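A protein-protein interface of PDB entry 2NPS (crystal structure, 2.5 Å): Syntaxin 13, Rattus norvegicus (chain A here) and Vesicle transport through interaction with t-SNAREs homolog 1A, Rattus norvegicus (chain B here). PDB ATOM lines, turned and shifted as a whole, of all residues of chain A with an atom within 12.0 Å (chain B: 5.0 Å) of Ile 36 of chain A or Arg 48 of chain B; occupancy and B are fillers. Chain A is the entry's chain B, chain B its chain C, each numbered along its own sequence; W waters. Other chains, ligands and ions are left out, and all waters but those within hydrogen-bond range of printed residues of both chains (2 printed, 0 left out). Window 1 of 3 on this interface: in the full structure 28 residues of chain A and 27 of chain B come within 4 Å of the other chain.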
ATOM      1  N   LEU A  25     -38.684 -24.560  -6.770  1.00  0.00           N
ATOM      2  CA  LEU A  25     -37.887 -23.618  -5.999  1.00  0.00           C
ATOM      3  C   LEU A  25     -36.823 -24.335  -5.187  1.00  0.00           C
ATOM      4  O   LEU A  25     -35.661 -23.939  -5.189  1.00  0.00           O
ATOM      5  CB  LEU A  25     -38.783 -22.801  -5.073  1.00  0.00           C
ATOM      6  CG  LEU A  25     -38.164 -21.540  -4.469  1.00  0.00           C
ATOM      7  CD1 LEU A  25     -37.914 -20.502  -5.567  1.00  0.00           C
ATOM      8  CD2 LEU A  25     -39.087 -20.965  -3.399  1.00  0.00           C
ATOM      9  N   ALA A  26     -37.227 -25.396  -4.496  1.00  0.00           N
ATOM     10  CA  ALA A  26     -36.308 -26.176  -3.675  1.00  0.00           C
ATOM     11  C   ALA A  26     -35.136 -26.664  -4.516  1.00  0.00           C
ATOM     12  O   ALA A  26     -33.983 -26.572  -4.106  1.00  0.00           O
ATOM     13  CB  ALA A  26     -37.035 -27.361  -3.059  1.00  0.00           C
ATOM     14  N   MET A  27     -35.443 -27.184  -5.697  1.00  0.00           N
ATOM     15  CA  MET A  27     -34.439 -27.693  -6.628  1.00  0.00           C
ATOM     16  C   MET A  27     -33.457 -26.585  -7.008  1.00  0.00           C
ATOM     17  O   MET A  27     -32.248 -26.771  -6.938  1.00  0.00           O
ATOM     18  CB  MET A  27     -35.155 -28.229  -7.867  1.00  0.00           C
ATOM     19  CG  MET A  27     -34.296 -28.483  -9.074  1.00  0.00           C
ATOM     20  SD  MET A  27     -35.366 -28.632 -10.522  1.00  0.00           S
ATOM     21  CE  MET A  27     -35.472 -26.877 -11.014  1.00  0.00           C
ATOM     22  N   MET A  28     -33.983 -25.428  -7.401  1.00  0.00           N
ATOM     23  CA  MET A  28     -33.139 -24.305  -7.776  1.00  0.00           C
ATOM     24  C   MET A  28     -32.199 -23.882  -6.661  1.00  0.00           C
ATOM     25  O   MET A  28     -31.012 -23.658  -6.897  1.00  0.00           O
ATOM     26  CB  MET A  28     -33.993 -23.119  -8.177  1.00  0.00           C
ATOM     27  CG  MET A  28     -34.742 -23.306  -9.464  1.00  0.00           C
ATOM     28  SD  MET A  28     -35.370 -21.737 -10.050  1.00  0.00           S
ATOM     29  CE  MET A  28     -36.791 -21.555  -8.982  1.00  0.00           C
ATOM     30  N   ILE A  29     -32.736 -23.769  -5.451  1.00  0.00           N
ATOM     31  CA  ILE A  29     -31.947 -23.368  -4.301  1.00  0.00           C
ATOM     32  C   ILE A  29     -30.876 -24.409  -4.009  1.00  0.00           C
ATOM     33  O   ILE A  29     -29.736 -24.077  -3.697  1.00  0.00           O
ATOM     34  CB  ILE A  29     -32.848 -23.165  -3.054  1.00  0.00           C
ATOM     35  CG1 ILE A  29     -33.750 -21.947  -3.262  1.00  0.00           C
ATOM     36  CG2 ILE A  29     -31.992 -22.977  -1.788  1.00  0.00           C
ATOM     37  CD1 ILE A  29     -34.691 -21.672  -2.124  1.00  0.00           C
ATOM     38  N   HIS A  30     -31.235 -25.678  -4.123  1.00  0.00           N
ATOM     39  CA  HIS A  30     -30.272 -26.735  -3.853  1.00  0.00           C
ATOM     40  C   HIS A  30     -29.128 -26.765  -4.851  1.00  0.00           C
ATOM     41  O   HIS A  30     -27.987 -27.015  -4.486  1.00  0.00           O
ATOM     42  CB  HIS A  30     -30.967 -28.094  -3.825  1.00  0.00           C
ATOM     43  CG  HIS A  30     -30.022 -29.249  -3.728  1.00  0.00           C
ATOM     44  ND1 HIS A  30     -29.308 -29.718  -4.813  1.00  0.00           N
ATOM     45  CD2 HIS A  30     -29.639 -30.003  -2.671  1.00  0.00           C
ATOM     46  CE1 HIS A  30     -28.526 -30.710  -4.427  1.00  0.00           C
ATOM     47  NE2 HIS A  30     -28.709 -30.903  -3.131  1.00  0.00           N
ATOM     48  N   ASP A  31     -29.435 -26.503  -6.112  1.00  0.00           N
ATOM     49  CA  ASP A  31     -28.417 -26.517  -7.145  1.00  0.00           C
ATOM     50  C   ASP A  31     -27.441 -25.350  -7.030  1.00  0.00           C
ATOM     51  O   ASP A  31     -26.288 -25.452  -7.436  1.00  0.00           O
ATOM     52  CB  ASP A  31     -29.092 -26.522  -8.521  1.00  0.00           C
ATOM     53  CG  ASP A  31     -29.841 -27.823  -8.803  1.00  0.00           C
ATOM     54  OD1 ASP A  31     -30.753 -27.822  -9.661  1.00  0.00           O
ATOM     55  OD2 ASP A  31     -29.503 -28.857  -8.172  1.00  0.00           O
ATOM     56  N   GLN A  32     -27.901 -24.241  -6.466  1.00  0.00           N
ATOM     57  CA  GLN A  32     -27.057 -23.066  -6.290  1.00  0.00           C
ATOM     58  C   GLN A  32     -26.026 -23.265  -5.202  1.00  0.00           C
ATOM     59  O   GLN A  32     -25.018 -22.564  -5.146  1.00  0.00           O
ATOM     60  CB  GLN A  32     -27.916 -21.844  -5.998  1.00  0.00           C
ATOM     61  CG  GLN A  32     -28.706 -21.451  -7.217  1.00  0.00           C
ATOM     62  CD  GLN A  32     -29.650 -20.303  -6.995  1.00  0.00           C
ATOM     63  OE1 GLN A  32     -29.906 -19.885  -5.864  1.00  0.00           O
ATOM     64  NE2 GLN A  32     -30.194 -19.791  -8.080  1.00  0.00           N
ATOM     65  N   GLY A  33     -26.275 -24.244  -4.345  1.00  0.00           N
ATOM     66  CA  GLY A  33     -25.343 -24.544  -3.280  1.00  0.00           C
ATOM     67  C   GLY A  33     -23.995 -24.972  -3.824  1.00  0.00           C
ATOM     68  O   GLY A  33     -23.016 -24.995  -3.085  1.00  0.00           O
ATOM     69  N   ASP A  34     -23.929 -25.321  -5.109  1.00  0.00           N
ATOM     70  CA  ASP A  34     -22.659 -25.722  -5.703  1.00  0.00           C
ATOM     71  C   ASP A  34     -21.905 -24.448  -6.070  1.00  0.00           C
ATOM     72  O   ASP A  34     -20.676 -24.425  -6.099  1.00  0.00           O
ATOM     73  CB  ASP A  34     -22.860 -26.567  -6.966  1.00  0.00           C
ATOM     74  CG  ASP A  34     -23.935 -27.636  -6.803  1.00  0.00           C
ATOM     75  OD1 ASP A  34     -23.890 -28.406  -5.807  1.00  0.00           O
ATOM     76  OD2 ASP A  34     -24.823 -27.712  -7.692  1.00  0.00           O
ATOM     77  N   LEU A  35     -22.646 -23.391  -6.379  1.00  0.00           N
ATOM     78  CA  LEU A  35     -22.003 -22.124  -6.677  1.00  0.00           C
ATOM     79  C   LEU A  35     -21.370 -21.664  -5.354  1.00  0.00           C
ATOM     80  O   LEU A  35     -20.224 -21.226  -5.310  1.00  0.00           O
ATOM     81  CB  LEU A  35     -23.034 -21.101  -7.166  1.00  0.00           C
ATOM     82  CG  LEU A  35     -23.672 -21.368  -8.532  1.00  0.00           C
ATOM     83  CD1 LEU A  35     -24.670 -20.288  -8.887  1.00  0.00           C
ATOM     84  CD2 LEU A  35     -22.587 -21.432  -9.590  1.00  0.00           C
ATOM     85  N   ILE A  36     -22.125 -21.799  -4.271  1.00  0.00           N
ATOM     86  CA  ILE A  36     -21.640 -21.418  -2.952  1.00  0.00           C
ATOM     87  C   ILE A  36     -20.411 -22.227  -2.558  1.00  0.00           C
ATOM     88  O   ILE A  36     -19.532 -21.731  -1.853  1.00  0.00           O
ATOM     89  CB  ILE A  36     -22.732 -21.596  -1.891  1.00  0.00           C
ATOM     90  CG1 ILE A  36     -23.854 -20.595  -2.170  1.00  0.00           C
ATOM     91  CG2 ILE A  36     -22.153 -21.404  -0.496  1.00  0.00           C
ATOM     92  CD1 ILE A  36     -25.134 -20.890  -1.462  1.00  0.00           C
ATOM     93  N   ASP A  37     -20.355 -23.473  -3.019  1.00  0.00           N
ATOM     94  CA  ASP A  37     -19.214 -24.346  -2.765  1.00  0.00           C
ATOM     95  C   ASP A  37     -17.968 -23.750  -3.417  1.00  0.00           C
ATOM     96  O   ASP A  37     -16.888 -23.745  -2.837  1.00  0.00           O
ATOM     97  CB  ASP A  37     -19.463 -25.735  -3.365  1.00  0.00           C
ATOM     98  CG  ASP A  37     -19.985 -26.735  -2.344  1.00  0.00           C
ATOM     99  OD1 ASP A  37     -21.070 -27.317  -2.584  1.00  0.00           O
ATOM    100  OD2 ASP A  37     -19.313 -26.945  -1.307  1.00  0.00           O
ATOM    101  N   SER A  38     -18.141 -23.242  -4.628  1.00  0.00           N
ATOM    102  CA  SER A  38     -17.055 -22.673  -5.399  1.00  0.00           C
ATOM    103  C   SER A  38     -16.542 -21.389  -4.797  1.00  0.00           C
ATOM    104  O   SER A  38     -15.342 -21.201  -4.628  1.00  0.00           O
ATOM    105  CB  SER A  38     -17.543 -22.396  -6.800  1.00  0.00           C
ATOM    106  OG  SER A  38     -18.215 -23.520  -7.310  1.00  0.00           O
ATOM    107  N   ILE A  39     -17.487 -20.506  -4.509  1.00  0.00           N
ATOM    108  CA  ILE A  39     -17.218 -19.213  -3.919  1.00  0.00           C
ATOM    109  C   ILE A  39     -16.448 -19.423  -2.631  1.00  0.00           C
ATOM    110  O   ILE A  39     -15.386 -18.846  -2.423  1.00  0.00           O
ATOM    111  CB  ILE A  39     -18.556 -18.503  -3.625  1.00  0.00           C
ATOM    112  CG1 ILE A  39     -19.259 -18.177  -4.945  1.00  0.00           C
ATOM    113  CG2 ILE A  39     -18.329 -17.264  -2.787  1.00  0.00           C
ATOM    114  CD1 ILE A  39     -20.744 -18.055  -4.822  1.00  0.00           C
ATOM    115  N   GLU A  40     -17.011 -20.271  -1.779  1.00  0.00           N
ATOM    116  CA  GLU A  40     -16.451 -20.631  -0.486  1.00  0.00           C
ATOM    117  C   GLU A  40     -15.031 -21.143  -0.626  1.00  0.00           C
ATOM    118  O   GLU A  40     -14.157 -20.758   0.134  1.00  0.00           O
ATOM    119  CB  GLU A  40     -17.337 -21.706   0.140  1.00  0.00           C
ATOM    120  CG  GLU A  40     -16.978 -22.146   1.539  1.00  0.00           C
ATOM    121  CD  GLU A  40     -18.220 -22.359   2.390  1.00  0.00           C
ATOM    122  OE1 GLU A  40     -19.116 -23.125   1.962  1.00  0.00           O
ATOM    123  OE2 GLU A  40     -18.301 -21.750   3.488  1.00  0.00           O
ATOM    124  N   ALA A  41     -14.807 -22.018  -1.595  1.00  0.00           N
ATOM    125  CA  ALA A  41     -13.489 -22.584  -1.824  1.00  0.00           C
ATOM    126  C   ALA A  41     -12.526 -21.538  -2.354  1.00  0.00           C
ATOM    127  O   ALA A  41     -11.362 -21.508  -1.972  1.00  0.00           O
ATOM    128  CB  ALA A  41     -13.589 -23.728  -2.799  1.00  0.00           C
ATOM    129  N   ASN A  42     -13.022 -20.686  -3.243  1.00  0.00           N
ATOM    130  CA  ASN A  42     -12.212 -19.634  -3.834  1.00  0.00           C
ATOM    131  C   ASN A  42     -11.695 -18.635  -2.817  1.00  0.00           C
ATOM    132  O   ASN A  42     -10.533 -18.266  -2.840  1.00  0.00           O
ATOM    133  CB  ASN A  42     -13.003 -18.914  -4.922  1.00  0.00           C
ATOM    134  CG  ASN A  42     -13.155 -19.754  -6.163  1.00  0.00           C
ATOM    135  OD1 ASN A  42     -12.177 -20.284  -6.666  1.00  0.00           O
ATOM    136  ND2 ASN A  42     -14.375 -19.884  -6.662  1.00  0.00           N
ATOM    137  N   VAL A  43     -12.572 -18.203  -1.924  1.00  0.00           N
ATOM    138  CA  VAL A  43     -12.187 -17.273  -0.877  1.00  0.00           C
ATOM    139  C   VAL A  43     -11.224 -17.953   0.080  1.00  0.00           C
ATOM    140  O   VAL A  43     -10.236 -17.363   0.493  1.00  0.00           O
ATOM    141  CB  VAL A  43     -13.411 -16.783  -0.104  1.00  0.00           C
ATOM    142  CG1 VAL A  43     -12.986 -16.075   1.160  1.00  0.00           C
ATOM    143  CG2 VAL A  43     -14.217 -15.853  -0.981  1.00  0.00           C
ATOM    144  N   GLU A  44     -11.511 -19.199   0.424  1.00  0.00           N
ATOM    145  CA  GLU A  44     -10.646 -19.956   1.309  1.00  0.00           C
ATOM    146  C   GLU A  44      -9.250 -19.946   0.741  1.00  0.00           C
ATOM    147  O   GLU A  44      -8.288 -19.601   1.419  1.00  0.00           O
ATOM    148  CB  GLU A  44     -11.100 -21.395   1.408  1.00  0.00           C
ATOM    149  CG  GLU A  44     -10.268 -22.169   2.394  1.00  0.00           C
ATOM    150  CD  GLU A  44     -10.398 -21.592   3.802  1.00  0.00           C
ATOM    151  OE1 GLU A  44      -9.512 -21.859   4.646  1.00  0.00           O
ATOM    152  OE2 GLU A  44     -11.397 -20.874   4.067  1.00  0.00           O
ATOM    153  N   SER A  45      -9.152 -20.323  -0.527  1.00  0.00           N
ATOM    154  CA  SER A  45      -7.883 -20.351  -1.226  1.00  0.00           C
ATOM    155  C   SER A  45      -7.199 -18.967  -1.197  1.00  0.00           C
ATOM    156  O   SER A  45      -5.997 -18.857  -0.942  1.00  0.00           O
ATOM    157  CB  SER A  45      -8.116 -20.803  -2.661  1.00  0.00           C
ATOM    158  OG  SER A  45      -6.888 -21.055  -3.297  1.00  0.00           O
ATOM    159  N   HIS B  44     -28.857 -22.320   5.912  1.00  0.00           N
ATOM    160  CA  HIS B  44     -27.559 -22.949   5.799  1.00  0.00           C
ATOM    161  C   HIS B  44     -26.672 -22.172   4.830  1.00  0.00           C
ATOM    162  O   HIS B  44     -25.492 -21.935   5.090  1.00  0.00           O
ATOM    163  CB  HIS B  44     -27.736 -24.383   5.307  1.00  0.00           C
ATOM    164  CG  HIS B  44     -26.626 -25.301   5.711  1.00  0.00           C
ATOM    165  ND1 HIS B  44     -26.567 -25.894   6.956  1.00  0.00           N
ATOM    166  CD2 HIS B  44     -25.514 -25.702   5.047  1.00  0.00           C
ATOM    167  CE1 HIS B  44     -25.464 -26.619   7.043  1.00  0.00           C
ATOM    168  NE2 HIS B  44     -24.807 -26.519   5.898  1.00  0.00           N
ATOM    169  N   ASP B  45     -27.251 -21.762   3.709  1.00  0.00           N
ATOM    170  CA  ASP B  45     -26.507 -21.010   2.711  1.00  0.00           C
ATOM    171  C   ASP B  45     -26.162 -19.639   3.258  1.00  0.00           C
ATOM    172  O   ASP B  45     -25.027 -19.185   3.134  1.00  0.00           O
ATOM    173  CB  ASP B  45     -27.331 -20.904   1.430  1.00  0.00           C
ATOM    174  CG  ASP B  45     -27.605 -22.263   0.813  1.00  0.00           C
ATOM    175  OD1 ASP B  45     -28.566 -22.384   0.023  1.00  0.00           O
ATOM    176  OD2 ASP B  45     -26.844 -23.215   1.121  1.00  0.00           O
ATOM    177  N   ARG B  46     -27.141 -19.001   3.887  1.00  0.00           N
ATOM    178  CA  ARG B  46     -26.935 -17.689   4.491  1.00  0.00           C
ATOM    179  C   ARG B  46     -25.780 -17.762   5.485  1.00  0.00           C
ATOM    180  O   ARG B  46     -25.032 -16.799   5.648  1.00  0.00           O
ATOM    181  CB  ARG B  46     -28.202 -17.230   5.217  1.00  0.00           C
ATOM    182  CG  ARG B  46     -28.047 -15.937   5.997  1.00  0.00           C
ATOM    183  CD  ARG B  46     -29.256 -15.691   6.909  1.00  0.00           C
ATOM    184  NE  ARG B  46     -29.248 -14.349   7.487  1.00  0.00           N
ATOM    185  CZ  ARG B  46     -30.000 -13.342   7.055  1.00  0.00           C
ATOM    186  NH1 ARG B  46     -29.918 -12.153   7.636  1.00  0.00           N
ATOM    187  NH2 ARG B  46     -30.844 -13.528   6.051  1.00  0.00           N
ATOM    188  N   GLU B  47     -25.637 -18.911   6.141  1.00  0.00           N
ATOM    189  CA  GLU B  47     -24.567 -19.094   7.102  1.00  0.00           C
ATOM    190  C   GLU B  47     -23.246 -19.186   6.346  1.00  0.00           C
ATOM    191  O   GLU B  47     -22.285 -18.508   6.694  1.00  0.00           O
ATOM    192  CB  GLU B  47     -24.817 -20.351   7.953  1.00  0.00           C
ATOM    193  CG  GLU B  47     -24.022 -20.389   9.279  1.00  0.00           C
ATOM    194  CD  GLU B  47     -24.762 -21.098  10.441  1.00  0.00           C
ATOM    195  OE1 GLU B  47     -24.271 -21.029  11.600  1.00  0.00           O
ATOM    196  OE2 GLU B  47     -25.826 -21.720  10.208  1.00  0.00           O
ATOM    197  N   ARG B  48     -23.206 -19.996   5.294  1.00  0.00           N
ATOM    198  CA  ARG B  48     -21.996 -20.154   4.493  1.00  0.00           C
ATOM    199  C   ARG B  48     -21.546 -18.841   3.818  1.00  0.00           C
ATOM    200  O   ARG B  48     -20.356 -18.568   3.703  1.00  0.00           O
ATOM    201  CB  ARG B  48     -22.225 -21.243   3.459  1.00  0.00           C
ATOM    202  CG  ARG B  48     -22.688 -22.542   4.074  1.00  0.00           C
ATOM    203  CD  ARG B  48     -23.223 -23.480   3.027  1.00  0.00           C
ATOM    204  NE  ARG B  48     -22.192 -23.857   2.068  1.00  0.00           N
ATOM    205  CZ  ARG B  48     -22.432 -24.468   0.917  1.00  0.00           C
ATOM    206  NH1 ARG B  48     -21.424 -24.778   0.115  1.00  0.00           N
ATOM    207  NH2 ARG B  48     -23.679 -24.756   0.565  1.00  0.00           N
ATOM    208  N   ILE B  49     -22.493 -18.022   3.383  1.00  0.00           N
ATOM    209  CA  ILE B  49     -22.145 -16.740   2.777  1.00  0.00           C
ATOM    210  C   ILE B  49     -21.529 -15.827   3.847  1.00  0.00           C
ATOM    211  O   ILE B  49     -20.556 -15.128   3.582  1.00  0.00           O
ATOM    212  CB  ILE B  49     -23.394 -16.022   2.184  1.00  0.00           C
ATOM    213  CG1 ILE B  49     -23.992 -16.842   1.037  1.00  0.00           C
ATOM    214  CG2 ILE B  49     -23.025 -14.621   1.713  1.00  0.00           C
ATOM    215  CD1 ILE B  49     -25.436 -16.479   0.732  1.00  0.00           C
ATOM    216  N   GLN B  50     -22.099 -15.820   5.051  1.00  0.00           N
ATOM    217  CA  GLN B  50     -21.563 -14.972   6.115  1.00  0.00           C
ATOM    218  C   GLN B  50     -20.190 -15.476   6.518  1.00  0.00           C
ATOM    219  O   GLN B  50     -19.286 -14.691   6.791  1.00  0.00           O
ATOM    220  CB  GLN B  50     -22.483 -14.944   7.341  1.00  0.00           C
ATOM    221  CG  GLN B  50     -23.873 -14.311   7.138  1.00  0.00           C
ATOM    222  CD  GLN B  50     -23.848 -12.865   6.628  1.00  0.00           C
ATOM    223  OE1 GLN B  50     -24.527 -11.983   7.166  1.00  0.00           O
ATOM    224  NE2 GLN B  50     -23.082 -12.625   5.584  1.00  0.00           N
ATOM    225  N   ARG B  51     -20.021 -16.787   6.546  1.00  0.00           N
ATOM    226  CA  ARG B  51     -18.731 -17.345   6.880  1.00  0.00           C
ATOM    227  C   ARG B  51     -17.684 -16.901   5.854  1.00  0.00           C
ATOM    228  O   ARG B  51     -16.556 -16.578   6.216  1.00  0.00           O
ATOM    229  CB  ARG B  51     -18.817 -18.860   6.910  1.00  0.00           C
ATOM    230  CG  ARG B  51     -19.150 -19.423   8.260  1.00  0.00           C
ATOM    231  CD  ARG B  51     -19.588 -20.860   8.149  1.00  0.00           C
ATOM    232  NE  ARG B  51     -18.723 -21.624   7.252  1.00  0.00           N
ATOM    233  CZ  ARG B  51     -19.062 -22.794   6.720  1.00  0.00           C
ATOM    234  NH1 ARG B  51     -20.244 -23.320   7.003  1.00  0.00           N
ATOM    235  NH2 ARG B  51     -18.237 -23.429   5.897  1.00  0.00           N
ATOM    236  N   ALA B  52     -18.070 -16.874   4.578  1.00  0.00           N
ATOM    237  CA  ALA B  52     -17.181 -16.479   3.481  1.00  0.00           C
ATOM    238  C   ALA B  52     -16.872 -15.000   3.510  1.00  0.00           C
ATOM    239  O   ALA B  52     -15.756 -14.591   3.223  1.00  0.00           O
ATOM    240  CB  ALA B  52     -17.801 -16.843   2.151  1.00  0.00           C
HETATM  241  O   HOH W   1     -27.860 -24.405  -1.408  1.00  0.00           O
HETATM  242  O   HOH W   2     -24.492 -27.182  -1.817  1.00  0.00           O
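NH1 of Arg 48 of chain B is in salt-bridge range of OD2 of Asp 37 of chain A, 3.3 Å away. The side-chain carboxylate of Glu 40 of chain A is in salt-bridge range of the guanidinium group of Arg 51 of chain B, 2.9 Å away. The side-chain carboxylate (OE1) of Glu 40 of chain A lies within salt-bridge range of the guanidinium group (NE) of Arg 48 of chain B, at 3.2 Å.
The side-chain carboxylate of Asp 45 of chain B lies within salt-bridge range of the guanidinium group of Arg 48 of chain B.
Among the printed residues, merely in contact across the chains: Ile 36 of chain A with Arg 48 of chain B, Gly 33 of chain A with Arg 48 of chain B, Ile 36 of chain A with Asp 45 of chain B, Val 43 of chain A with Ala 52 of chain B and Ile 29 of chain A with Asp 45 of chain B.
Of the printed residues of chain B, Gly 33 of chain A touches Arg 48. Ile 36 of chain A touches two residues of chain B. Of the printed residues of chain B, Glu 40 of chain A touches Arg 48 and Arg 51. Asp 45 of chain B touches just these residues of chain A: Ile 29 and Ile 36. No residue of chain A comes within 4 Å of Glu 47 of chain B. Of the printed residues of chain A, Arg 48 of chain B touches Gly 33, Ile 36, Asp 37 and Glu 40. Ile 49 of chain B touches none of the printed residues of chain A. Printed residues of chain A within 4 Å of Arg 51 of chain B: Glu 40 (2.9 Å).
Of the 21 printed residues of chain A, 6 touch a printed residue of chain B. Hydrophobic or aromatic side chains of chain A that line the printed part of chain B: Ile 29, Ile 36 and Val 43. Among the printed residues, 8 pairs touch across the chains.
Water W1 lies within hydrogen-bond range of the side-chain carboxylate (OD1) of Asp 45 of chain B (2.6 Å), the backbone carbonyl oxygen (O) of Ile 29 of chain A (3.0 Å) and the backbone NH (N) of Gly 33 of chain A (3.3 Å). Water W2 lies within hydrogen-bond range of O of Gly 33 of chain A (2.9 Å) and NH2 of Arg 48 of chain B (3.5 Å).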
